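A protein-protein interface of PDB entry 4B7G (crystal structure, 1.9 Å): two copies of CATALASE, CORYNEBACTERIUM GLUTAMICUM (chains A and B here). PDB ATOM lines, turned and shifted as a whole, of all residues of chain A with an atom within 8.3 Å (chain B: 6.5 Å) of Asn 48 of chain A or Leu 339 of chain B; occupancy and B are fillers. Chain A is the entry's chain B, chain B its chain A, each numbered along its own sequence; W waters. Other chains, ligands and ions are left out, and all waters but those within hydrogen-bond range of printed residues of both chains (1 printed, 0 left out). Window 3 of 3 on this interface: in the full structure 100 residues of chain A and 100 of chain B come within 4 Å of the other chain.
The backbone carbonyl oxygen (O) of Gln 346 of chain B lies close to the side-chain amide oxygen (OD1) of Asn 48 of chain A, at 2.9 Å. The backbone carbonyl oxygen (O) of Gly 331 of chain B lies within hydrogen-bond range of the guanidinium group (NH2) of Arg 24 of chain A, 2.9 Å away.
The backbone NH (N) of Leu 339 of chain B is in hydrogen-bond range of the backbone carbonyl oxygen (O) of Ile 428 of chain B, at 2.8 Å. The backbone carbonyl oxygen of Ser 340 of chain B lies within hydrogen-bond range of the side-chain amide nitrogen of Gln 346 of chain B (2.9 Å). The side-chain amide nitrogen (NE2) of Gln 346 of chain B is in hydrogen-bond range of the side-chain hydroxyl (OH) of Tyr 429 of chain B (3.1 Å). The backbone NH of Ala 37 of chain A sits at hydrogen-bond distance from the side-chain carboxylate of Asp 49 of chain A. The backbone NH (N) of Val 46 of chain A is in hydrogen-bond range of the backbone carbonyl oxygen (O) of Ala 37 of chain A, 3.1 Å away.
NH2 of Arg 24 of chain A touches O of Ile 333 of chain B, 3.6 Å away. Ala 37 of chain A touches Ile 428 of chain B (CB to CD1, 3.7 Å). O of Gln 346 of chain B touches CD2 of Leu 47 of chain A (3.5 Å). Leu 339 of chain B touches Asn 48 of chain A (CD1 to ND2, 3.7 Å). OD1 of Asn 48 of chain A touches CB of Ile 349 of chain B (3.4 Å). Ile 428 of chain B touches Asn 48 of chain A (CD1 to O, 3.7 Å). CD1 of Ile 50 of chain A touches O of Gly 331 of chain B, at 3.5 Å. Ile 50 of chain A touches Ile 333 of chain B. Ile 50 of chain A touches Ile 349 of chain B.
Printed residues of chain B within 4 Å of Arg 24 of chain A: Gly 331 (2.9 Å) and Ile 333 (3.6 Å). Val 46 of chain A touches none of the printed residues of chain B. Of the printed residues of chain B, Leu 47 of chain A touches Gln 346 (3.5 Å). Printed residues of chain A within 4 Å of Ile 333 of chain B: Arg 24 (3.6 Å) and Ile 50 (3.99 Å). No residue of chain A comes within 4 Å of Gly 338 of chain B. Of the printed residues of chain A, Leu 339 of chain B touches Asn 48 (3.7 Å). No residue of chain A comes within 4 Å of Ser 340 of chain B. Pro 341 of chain B touches none of the printed residues of chain A. Of the printed residues of chain A, Ile 349 of chain B touches Asn 48 and Ile 50.
Hydrophobic or aromatic side chains of chain A that line the printed part of chain B: Ala 37, Leu 47 and Ile 50. Hydrophobic or aromatic side chains of chain B within 4 Å of the printed part of chain A: Ile 333, Leu 339, Ile 349 and Ile 428. Among the printed residues, no Asp or Glu carboxylate lies within 4 Å of a Lys or Arg side-chain nitrogen of the other chain.
No position is printed for both chains.
Water W1 lies within hydrogen-bond range of the side-chain amide oxygen of Gln 346 of chain B (2.9 Å), the backbone NH of Asn 48 of chain A (3.0 Å) and the backbone NH of Leu 47 of chain A (3.2 Å).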
ATOM      1  N   ARG A  24      34.980  -3.312  -4.776  1.00  0.00           N
ATOM      2  CA  ARG A  24      35.617  -2.387  -5.708  1.00  0.00           C
ATOM      3  C   ARG A  24      37.108  -2.343  -5.425  1.00  0.00           C
ATOM      4  O   ARG A  24      37.592  -2.965  -4.463  1.00  0.00           O
ATOM      5  CB  ARG A  24      35.027  -0.983  -5.590  1.00  0.00           C
ATOM      6  CG  ARG A  24      33.522  -0.957  -5.736  1.00  0.00           C
ATOM      7  CD  ARG A  24      33.022   0.414  -6.207  1.00  0.00           C
ATOM      8  NE  ARG A  24      33.766   1.515  -5.608  1.00  0.00           N
ATOM      9  CZ  ARG A  24      33.441   2.123  -4.472  1.00  0.00           C
ATOM     10  NH1 ARG A  24      32.374   1.746  -3.774  1.00  0.00           N
ATOM     11  NH2 ARG A  24      34.195   3.120  -4.034  1.00  0.00           N
ATOM     12  N   ALA A  37      22.934   1.236 -12.212  1.00  0.00           N
ATOM     13  CA  ALA A  37      22.013   2.147 -11.524  1.00  0.00           C
ATOM     14  C   ALA A  37      21.433   3.199 -12.465  1.00  0.00           C
ATOM     15  O   ALA A  37      22.174   3.866 -13.193  1.00  0.00           O
ATOM     16  CB  ALA A  37      22.725   2.825 -10.340  1.00  0.00           C
ATOM     17  N   ASN A  45      20.861   6.061 -17.278  1.00  0.00           N
ATOM     18  CA  ASN A  45      21.919   5.567 -16.411  1.00  0.00           C
ATOM     19  C   ASN A  45      22.573   6.752 -15.728  1.00  0.00           C
ATOM     20  O   ASN A  45      22.821   7.783 -16.370  1.00  0.00           O
ATOM     21  CB  ASN A  45      22.973   4.813 -17.221  1.00  0.00           C
ATOM     22  CG  ASN A  45      22.672   3.342 -17.328  1.00  0.00           C
ATOM     23  OD1 ASN A  45      23.232   2.517 -16.591  1.00  0.00           O
ATOM     24  ND2 ASN A  45      21.782   2.998 -18.239  1.00  0.00           N
ATOM     25  N   VAL A  46      22.857   6.614 -14.437  1.00  0.00           N
ATOM     26  CA  VAL A  46      23.507   7.689 -13.692  1.00  0.00           C
ATOM     27  C   VAL A  46      25.026   7.637 -13.872  1.00  0.00           C
ATOM     28  O   VAL A  46      25.591   6.573 -14.140  1.00  0.00           O
ATOM     29  CB  VAL A  46      23.141   7.656 -12.191  1.00  0.00           C
ATOM     30  CG1 VAL A  46      21.630   7.680 -12.013  1.00  0.00           C
ATOM     31  CG2 VAL A  46      23.743   6.432 -11.496  1.00  0.00           C
ATOM     32  N   LEU A  47      25.670   8.794 -13.756  1.00  0.00           N
ATOM     33  CA  LEU A  47      27.117   8.885 -13.870  1.00  0.00           C
ATOM     34  C   LEU A  47      27.767   8.141 -12.711  1.00  0.00           C
ATOM     35  O   LEU A  47      28.757   7.419 -12.889  1.00  0.00           O
ATOM     36  CB  LEU A  47      27.550  10.361 -13.850  1.00  0.00           C
ATOM     37  CG  LEU A  47      29.054  10.671 -13.920  1.00  0.00           C
ATOM     38  CD1 LEU A  47      29.662  10.123 -15.211  1.00  0.00           C
ATOM     39  CD2 LEU A  47      29.287  12.175 -13.826  1.00  0.00           C
ATOM     40  N   ASN A  48      27.200   8.300 -11.520  1.00  0.00           N
ATOM     41  CA  ASN A  48      27.872   7.800 -10.329  1.00  0.00           C
ATOM     42  C   ASN A  48      27.557   6.364  -9.956  1.00  0.00           C
ATOM     43  O   ASN A  48      27.392   6.062  -8.769  1.00  0.00           O
ATOM     44  CB  ASN A  48      27.596   8.704  -9.133  1.00  0.00           C
ATOM     45  CG  ASN A  48      28.076  10.106  -9.350  1.00  0.00           C
ATOM     46  OD1 ASN A  48      28.990  10.370 -10.148  1.00  0.00           O
ATOM     47  ND2 ASN A  48      27.474  11.025  -8.632  1.00  0.00           N
ATOM     48  N   ASP A  49      27.486   5.480 -10.948  1.00  0.00           N
ATOM     49  CA  ASP A  49      27.568   4.057 -10.650  1.00  0.00           C
ATOM     50  C   ASP A  49      29.063   3.784 -10.651  1.00  0.00           C
ATOM     51  O   ASP A  49      29.661   3.531 -11.707  1.00  0.00           O
ATOM     52  CB  ASP A  49      26.837   3.199 -11.692  1.00  0.00           C
ATOM     53  CG  ASP A  49      26.712   1.737 -11.262  1.00  0.00           C
ATOM     54  OD1 ASP A  49      27.642   1.242 -10.579  1.00  0.00           O
ATOM     55  OD2 ASP A  49      25.697   1.075 -11.601  1.00  0.00           O
ATOM     56  N   ILE A  50      29.675   3.885  -9.472  1.00  0.00           N
ATOM     57  CA  ILE A  50      31.134   3.870  -9.369  1.00  0.00           C
ATOM     58  C   ILE A  50      31.711   2.533  -9.830  1.00  0.00           C
ATOM     59  O   ILE A  50      32.698   2.497 -10.575  1.00  0.00           O
ATOM     60  CB  ILE A  50      31.609   4.193  -7.926  1.00  0.00           C
ATOM     61  CG1 ILE A  50      31.070   5.552  -7.481  1.00  0.00           C
ATOM     62  CG2 ILE A  50      33.125   4.230  -7.863  1.00  0.00           C
ATOM     63  CD1 ILE A  50      31.231   5.838  -5.974  1.00  0.00           C
ATOM     64  N   HIS A  51      31.099   1.434  -9.402  1.00  0.00           N
ATOM     65  CA  HIS A  51      31.570   0.118  -9.830  1.00  0.00           C
ATOM     66  C   HIS A  51      31.443  -0.043 -11.354  1.00  0.00           C
ATOM     67  O   HIS A  51      32.369  -0.540 -12.021  1.00  0.00           O
ATOM     68  CB  HIS A  51      30.813  -1.003  -9.096  1.00  0.00           C
ATOM     69  CG  HIS A  51      31.239  -2.383  -9.507  1.00  0.00           C
ATOM     70  ND1 HIS A  51      32.548  -2.812  -9.427  1.00  0.00           N
ATOM     71  CD2 HIS A  51      30.536  -3.415 -10.029  1.00  0.00           C
ATOM     72  CE1 HIS A  51      32.629  -4.055  -9.864  1.00  0.00           C
ATOM     73  NE2 HIS A  51      31.422  -4.447 -10.237  1.00  0.00           N
ATOM     74  N   LEU A  52      30.316   0.378 -11.920  1.00  0.00           N
ATOM     75  CA  LEU A  52      30.139   0.237 -13.367  1.00  0.00           C
ATOM     76  C   LEU A  52      31.288   0.880 -14.130  1.00  0.00           C
ATOM     77  O   LEU A  52      31.927   0.247 -14.976  1.00  0.00           O
ATOM     78  CB  LEU A  52      28.814   0.857 -13.827  1.00  0.00           C
ATOM     79  CG  LEU A  52      28.651   0.934 -15.344  1.00  0.00           C
ATOM     80  CD1 LEU A  52      28.469  -0.453 -15.939  1.00  0.00           C
ATOM     81  CD2 LEU A  52      27.467   1.853 -15.733  1.00  0.00           C
ATOM     82  N   ILE A  53      31.554   2.143 -13.823  1.00  0.00           N
ATOM     83  CA  ILE A  53      32.606   2.879 -14.511  1.00  0.00           C
ATOM     84  C   ILE A  53      33.978   2.255 -14.260  1.00  0.00           C
ATOM     85  O   ILE A  53      34.782   2.119 -15.181  1.00  0.00           O
ATOM     86  CB  ILE A  53      32.595   4.365 -14.113  1.00  0.00           C
ATOM     87  CG1 ILE A  53      31.216   4.960 -14.412  1.00  0.00           C
ATOM     88  CG2 ILE A  53      33.699   5.144 -14.859  1.00  0.00           C
ATOM     89  CD1 ILE A  53      30.764   4.719 -15.865  1.00  0.00           C
ATOM     90  N   THR B 213      28.155  18.738   0.674  1.00  0.00           N
ATOM     91  CA  THR B 213      27.222  17.922   1.452  1.00  0.00           C
ATOM     92  C   THR B 213      27.407  16.467   1.046  1.00  0.00           C
ATOM     93  O   THR B 213      27.369  16.126  -0.146  1.00  0.00           O
ATOM     94  CB  THR B 213      25.782  18.344   1.156  1.00  0.00           C
ATOM     95  OG1 THR B 213      25.617  19.719   1.534  1.00  0.00           O
ATOM     96  CG2 THR B 213      24.776  17.473   1.912  1.00  0.00           C
ATOM     97  N   PHE B 214      27.643  15.606   2.028  1.00  0.00           N
ATOM     98  CA  PHE B 214      27.631  14.166   1.784  1.00  0.00           C
ATOM     99  C   PHE B 214      26.458  13.576   2.533  1.00  0.00           C
ATOM    100  O   PHE B 214      25.681  14.315   3.150  1.00  0.00           O
ATOM    101  CB  PHE B 214      28.931  13.524   2.262  1.00  0.00           C
ATOM    102  CG  PHE B 214      30.129  13.950   1.467  1.00  0.00           C
ATOM    103  CD1 PHE B 214      30.460  13.296   0.284  1.00  0.00           C
ATOM    104  CD2 PHE B 214      30.913  15.025   1.887  1.00  0.00           C
ATOM    105  CE1 PHE B 214      31.573  13.697  -0.462  1.00  0.00           C
ATOM    106  CE2 PHE B 214      32.017  15.433   1.151  1.00  0.00           C
ATOM    107  CZ  PHE B 214      32.345  14.768  -0.027  1.00  0.00           C
ATOM    108  N   GLN B 215      26.322  12.253   2.492  1.00  0.00           N
ATOM    109  CA  GLN B 215      25.260  11.595   3.251  1.00  0.00           C
ATOM    110  C   GLN B 215      25.843  10.586   4.237  1.00  0.00           C
ATOM    111  O   GLN B 215      26.831   9.905   3.934  1.00  0.00           O
ATOM    112  CB  GLN B 215      24.278  10.891   2.301  1.00  0.00           C
ATOM    113  CG  GLN B 215      22.923  10.579   2.936  1.00  0.00           C
ATOM    114  CD  GLN B 215      21.914  10.086   1.920  1.00  0.00           C
ATOM    115  OE1 GLN B 215      21.071  10.855   1.434  1.00  0.00           O
ATOM    116  NE2 GLN B 215      21.998   8.804   1.581  1.00  0.00           N
ATOM    117  N   TRP B 225      21.985  14.321   5.999  1.00  0.00           N
ATOM    118  CA  TRP B 225      23.018  15.027   5.239  1.00  0.00           C
ATOM    119  C   TRP B 225      24.108  15.554   6.179  1.00  0.00           C
ATOM    120  O   TRP B 225      23.806  16.027   7.280  1.00  0.00           O
ATOM    121  CB  TRP B 225      22.406  16.190   4.449  1.00  0.00           C
ATOM    122  CG  TRP B 225      21.279  15.795   3.525  1.00  0.00           C
ATOM    123  CD1 TRP B 225      19.948  16.078   3.687  1.00  0.00           C
ATOM    124  CD2 TRP B 225      21.384  15.062   2.291  1.00  0.00           C
ATOM    125  NE1 TRP B 225      19.225  15.568   2.632  1.00  0.00           N
ATOM    126  CE2 TRP B 225      20.082  14.936   1.769  1.00  0.00           C
ATOM    127  CE3 TRP B 225      22.454  14.500   1.582  1.00  0.00           C
ATOM    128  CZ2 TRP B 225      19.822  14.274   0.559  1.00  0.00           C
ATOM    129  CZ3 TRP B 225      22.191  13.836   0.387  1.00  0.00           C
ATOM    130  CH2 TRP B 225      20.890  13.731  -0.111  1.00  0.00           C
ATOM    131  N   PRO B 330      37.551  11.117  -4.306  1.00  0.00           N
ATOM    132  CA  PRO B 330      36.339  11.238  -3.490  1.00  0.00           C
ATOM    133  C   PRO B 330      35.351  10.117  -3.780  1.00  0.00           C
ATOM    134  O   PRO B 330      34.424   9.902  -2.987  1.00  0.00           O
ATOM    135  CB  PRO B 330      35.748  12.592  -3.921  1.00  0.00           C
ATOM    136  CG  PRO B 330      36.316  12.829  -5.315  1.00  0.00           C
ATOM    137  CD  PRO B 330      37.698  12.235  -5.258  1.00  0.00           C
ATOM    138  N   GLY B 331      35.540   9.411  -4.894  1.00  0.00           N
ATOM    139  CA  GLY B 331      34.723   8.245  -5.199  1.00  0.00           C
ATOM    140  C   GLY B 331      35.060   7.041  -4.336  1.00  0.00           C
ATOM    141  O   GLY B 331      34.361   6.019  -4.367  1.00  0.00           O
ATOM    142  N   ILE B 333      34.337   5.813  -1.522  1.00  0.00           N
ATOM    143  CA  ILE B 333      33.424   5.842  -0.387  1.00  0.00           C
ATOM    144  C   ILE B 333      33.226   4.421   0.129  1.00  0.00           C
ATOM    145  O   ILE B 333      33.627   3.454  -0.526  1.00  0.00           O
ATOM    146  CB  ILE B 333      32.073   6.492  -0.750  1.00  0.00           C
ATOM    147  CG1 ILE B 333      31.370   5.697  -1.859  1.00  0.00           C
ATOM    148  CG2 ILE B 333      32.286   7.953  -1.177  1.00  0.00           C
ATOM    149  CD1 ILE B 333      29.989   6.236  -2.207  1.00  0.00           C
ATOM    150  N   VAL B 337      28.359   5.823   4.095  1.00  0.00           N
ATOM    151  CA  VAL B 337      28.637   7.137   3.530  1.00  0.00           C
ATOM    152  C   VAL B 337      28.073   7.197   2.108  1.00  0.00           C
ATOM    153  O   VAL B 337      28.210   6.234   1.338  1.00  0.00           O
ATOM    154  CB  VAL B 337      30.152   7.403   3.465  1.00  0.00           C
ATOM    155  CG1 VAL B 337      30.435   8.702   2.723  1.00  0.00           C
ATOM    156  CG2 VAL B 337      30.760   7.432   4.867  1.00  0.00           C
ATOM    157  N   GLY B 338      27.445   8.317   1.757  1.00  0.00           N
ATOM    158  CA  GLY B 338      26.922   8.490   0.411  1.00  0.00           C
ATOM    159  C   GLY B 338      27.160   9.879  -0.163  1.00  0.00           C
ATOM    160  O   GLY B 338      27.717  10.768   0.496  1.00  0.00           O
ATOM    161  N   LEU B 339      26.725  10.066  -1.403  1.00  0.00           N
ATOM    162  CA  LEU B 339      26.904  11.331  -2.092  1.00  0.00           C
ATOM    163  C   LEU B 339      25.668  12.223  -1.893  1.00  0.00           C
ATOM    164  O   LEU B 339      24.929  12.070  -0.908  1.00  0.00           O
ATOM    165  CB  LEU B 339      27.165  11.063  -3.575  1.00  0.00           C
ATOM    166  CG  LEU B 339      28.221   9.983  -3.848  1.00  0.00           C
ATOM    167  CD1 LEU B 339      28.303   9.647  -5.336  1.00  0.00           C
ATOM    168  CD2 LEU B 339      29.583  10.417  -3.324  1.00  0.00           C
ATOM    169  N   SER B 340      25.452  13.155  -2.813  1.00  0.00           N
ATOM    170  CA  SER B 340      24.314  14.074  -2.743  1.00  0.00           C
ATOM    171  C   SER B 340      24.156  14.696  -4.123  1.00  0.00           C
ATOM    172  O   SER B 340      25.048  14.556  -4.965  1.00  0.00           O
ATOM    173  CB  SER B 340      24.573  15.165  -1.701  1.00  0.00           C
ATOM    174  OG  SER B 340      25.496  16.125  -2.203  1.00  0.00           O
ATOM    175  N   PRO B 341      23.020  15.369  -4.379  1.00  0.00           N
ATOM    176  CA  PRO B 341      22.868  16.015  -5.691  1.00  0.00           C
ATOM    177  C   PRO B 341      23.640  17.329  -5.822  1.00  0.00           C
ATOM    178  O   PRO B 341      23.091  18.332  -6.294  1.00  0.00           O
ATOM    179  CB  PRO B 341      21.354  16.265  -5.795  1.00  0.00           C
ATOM    180  CG  PRO B 341      20.870  16.285  -4.390  1.00  0.00           C
ATOM    181  CD  PRO B 341      21.748  15.333  -3.626  1.00  0.00           C
ATOM    182  N   ASP B 342      24.901  17.310  -5.400  1.00  0.00           N
ATOM    183  CA  ASP B 342      25.850  18.393  -5.652  1.00  0.00           C
ATOM    184  C   ASP B 342      26.526  18.051  -6.983  1.00  0.00           C
ATOM    185  O   ASP B 342      27.268  17.058  -7.056  1.00  0.00           O
ATOM    186  CB  ASP B 342      26.877  18.406  -4.510  1.00  0.00           C
ATOM    187  CG  ASP B 342      27.948  19.479  -4.666  1.00  0.00           C
ATOM    188  OD1 ASP B 342      28.362  19.796  -5.812  1.00  0.00           O
ATOM    189  OD2 ASP B 342      28.410  19.992  -3.620  1.00  0.00           O
ATOM    190  N   LEU B 345      30.283  17.613  -7.038  1.00  0.00           N
ATOM    191  CA  LEU B 345      30.657  16.347  -6.422  1.00  0.00           C
ATOM    192  C   LEU B 345      30.461  15.196  -7.391  1.00  0.00           C
ATOM    193  O   LEU B 345      31.351  14.347  -7.532  1.00  0.00           O
ATOM    194  CB  LEU B 345      29.823  16.109  -5.164  1.00  0.00           C
ATOM    195  CG  LEU B 345      29.997  14.750  -4.494  1.00  0.00           C
ATOM    196  CD1 LEU B 345      31.470  14.500  -4.116  1.00  0.00           C
ATOM    197  CD2 LEU B 345      29.090  14.676  -3.270  1.00  0.00           C
ATOM    198  N   GLN B 346      29.318  15.168  -8.075  1.00  0.00           N
ATOM    199  CA  GLN B 346      29.033  14.045  -8.970  1.00  0.00           C
ATOM    200  C   GLN B 346      30.001  13.970 -10.149  1.00  0.00           C
ATOM    201  O   GLN B 346      30.353  12.878 -10.607  1.00  0.00           O
ATOM    202  CB  GLN B 346      27.576  14.068  -9.433  1.00  0.00           C
ATOM    203  CG  GLN B 346      26.617  14.024  -8.248  1.00  0.00           C
ATOM    204  CD  GLN B 346      25.296  13.353  -8.554  1.00  0.00           C
ATOM    205  OE1 GLN B 346      25.010  12.966  -9.699  1.00  0.00           O
ATOM    206  NE2 GLN B 346      24.467  13.211  -7.516  1.00  0.00           N
ATOM    207  N   ALA B 347      30.433  15.126 -10.638  1.00  0.00           N
ATOM    208  CA  ALA B 347      31.479  15.167 -11.657  1.00  0.00           C
ATOM    209  C   ALA B 347      32.811  14.651 -11.113  1.00  0.00           C
ATOM    210  O   ALA B 347      33.518  13.908 -11.810  1.00  0.00           O
ATOM    211  CB  ALA B 347      31.643  16.577 -12.203  1.00  0.00           C
ATOM    212  N   ARG B 348      33.173  15.062  -9.894  1.00  0.00           N
ATOM    213  CA  ARG B 348      34.426  14.598  -9.260  1.00  0.00           C
ATOM    214  C   ARG B 348      34.475  13.072  -9.112  1.00  0.00           C
ATOM    215  O   ARG B 348      35.537  12.446  -9.263  1.00  0.00           O
ATOM    216  CB  ARG B 348      34.610  15.238  -7.873  1.00  0.00           C
ATOM    217  CG  ARG B 348      34.735  16.760  -7.878  1.00  0.00           C
ATOM    218  CD  ARG B 348      34.895  17.303  -6.445  1.00  0.00           C
ATOM    219  NE  ARG B 348      36.190  16.923  -5.871  1.00  0.00           N
ATOM    220  CZ  ARG B 348      36.396  16.703  -4.575  1.00  0.00           C
ATOM    221  NH1 ARG B 348      35.392  16.823  -3.714  1.00  0.00           N
ATOM    222  NH2 ARG B 348      37.602  16.354  -4.138  1.00  0.00           N
ATOM    223  N   ILE B 349      33.326  12.474  -8.811  1.00  0.00           N
ATOM    224  CA  ILE B 349      33.260  11.023  -8.619  1.00  0.00           C
ATOM    225  C   ILE B 349      33.778  10.299  -9.867  1.00  0.00           C
ATOM    226  O   ILE B 349      34.428   9.244  -9.767  1.00  0.00           O
ATOM    227  CB  ILE B 349      31.835  10.554  -8.218  1.00  0.00           C
ATOM    228  CG1 ILE B 349      31.388  11.200  -6.893  1.00  0.00           C
ATOM    229  CG2 ILE B 349      31.753   9.026  -8.135  1.00  0.00           C
ATOM    230  CD1 ILE B 349      32.317  10.920  -5.689  1.00  0.00           C
ATOM    231  N   PHE B 350      33.528  10.878 -11.040  1.00  0.00           N
ATOM    232  CA  PHE B 350      34.130  10.368 -12.269  1.00  0.00           C
ATOM    233  C   PHE B 350      35.607  10.757 -12.441  1.00  0.00           C
ATOM    234  O   PHE B 350      36.452   9.915 -12.761  1.00  0.00           O
ATOM    235  CB  PHE B 350      33.356  10.856 -13.502  1.00  0.00           C
ATOM    236  CG  PHE B 350      34.118  10.674 -14.790  1.00  0.00           C
ATOM    237  CD1 PHE B 350      34.268   9.411 -15.346  1.00  0.00           C
ATOM    238  CD2 PHE B 350      34.702  11.758 -15.431  1.00  0.00           C
ATOM    239  CE1 PHE B 350      34.985   9.231 -16.530  1.00  0.00           C
ATOM    240  CE2 PHE B 350      35.418  11.588 -16.611  1.00  0.00           C
ATOM    241  CZ  PHE B 350      35.565  10.323 -17.159  1.00  0.00           C
ATOM    242  N   ASP B 426      20.889   3.003  -2.190  1.00  0.00           N
ATOM    243  CA  ASP B 426      21.274   3.817  -1.036  1.00  0.00           C
ATOM    244  C   ASP B 426      22.786   3.938  -0.852  1.00  0.00           C
ATOM    245  O   ASP B 426      23.265   4.901  -0.243  1.00  0.00           O
ATOM    246  CB  ASP B 426      20.636   3.263   0.247  1.00  0.00           C
ATOM    247  CG  ASP B 426      21.005   1.812   0.499  1.00  0.00           C
ATOM    248  OD1 ASP B 426      20.848   0.995  -0.427  1.00  0.00           O
ATOM    249  OD2 ASP B 426      21.464   1.488   1.618  1.00  0.00           O
ATOM    250  N   ASP B 427      23.527   2.955  -1.358  1.00  0.00           N
ATOM    251  CA  ASP B 427      24.990   2.981  -1.322  1.00  0.00           C
ATOM    252  C   ASP B 427      25.570   4.132  -2.153  1.00  0.00           C
ATOM    253  O   ASP B 427      26.716   4.553  -1.946  1.00  0.00           O
ATOM    254  CB  ASP B 427      25.525   1.660  -1.849  1.00  0.00           C
ATOM    255  CG  ASP B 427      25.050   1.375  -3.244  1.00  0.00           C
ATOM    256  OD1 ASP B 427      23.884   0.952  -3.403  1.00  0.00           O
ATOM    257  OD2 ASP B 427      25.835   1.587  -4.194  1.00  0.00           O
ATOM    258  N   ILE B 428      24.790   4.623  -3.113  1.00  0.00           N
ATOM    259  CA  ILE B 428      25.171   5.834  -3.847  1.00  0.00           C
ATOM    260  C   ILE B 428      24.690   7.042  -3.043  1.00  0.00           C
ATOM    261  O   ILE B 428      25.505   7.797  -2.501  1.00  0.00           O
ATOM    262  CB  ILE B 428      24.596   5.842  -5.263  1.00  0.00           C
ATOM    263  CG1 ILE B 428      24.974   4.542  -5.984  1.00  0.00           C
ATOM    264  CG2 ILE B 428      25.101   7.049  -6.025  1.00  0.00           C
ATOM    265  CD1 ILE B 428      24.398   4.405  -7.395  1.00  0.00           C
ATOM    266  N   TYR B 429      23.372   7.215  -2.968  1.00  0.00           N
ATOM    267  CA  TYR B 429      22.739   7.972  -1.875  1.00  0.00           C
ATOM    268  C   TYR B 429      21.239   7.737  -1.873  1.00  0.00           C
ATOM    269  O   TYR B 429      20.661   7.371  -2.900  1.00  0.00           O
ATOM    270  CB  TYR B 429      23.043   9.485  -1.911  1.00  0.00           C
ATOM    271  CG  TYR B 429      22.664  10.200  -3.191  1.00  0.00           C
ATOM    272  CD1 TYR B 429      23.446  10.070  -4.334  1.00  0.00           C
ATOM    273  CD2 TYR B 429      21.549  11.031  -3.250  1.00  0.00           C
ATOM    274  CE1 TYR B 429      23.119  10.721  -5.509  1.00  0.00           C
ATOM    275  CE2 TYR B 429      21.207  11.699  -4.433  1.00  0.00           C
ATOM    276  CZ  TYR B 429      22.004  11.535  -5.559  1.00  0.00           C
ATOM    277  OH  TYR B 429      21.693  12.186  -6.748  1.00  0.00           O
ATOM    278  N   VAL B 430      20.606   7.924  -0.718  1.00  0.00           N
ATOM    279  CA  VAL B 430      19.151   8.020  -0.703  1.00  0.00           C
ATOM    280  C   VAL B 430      18.816   9.385  -1.282  1.00  0.00           C
ATOM    281  O   VAL B 430      19.163  10.416  -0.696  1.00  0.00           O
ATOM    282  CB  VAL B 430      18.573   7.880   0.719  1.00  0.00           C
ATOM    283  CG1 VAL B 430      17.036   7.881   0.674  1.00  0.00           C
ATOM    284  CG2 VAL B 430      19.071   6.595   1.352  1.00  0.00           C
HETATM  285  O   HOH W   1      25.190  10.412 -11.027  1.00  0.00           O
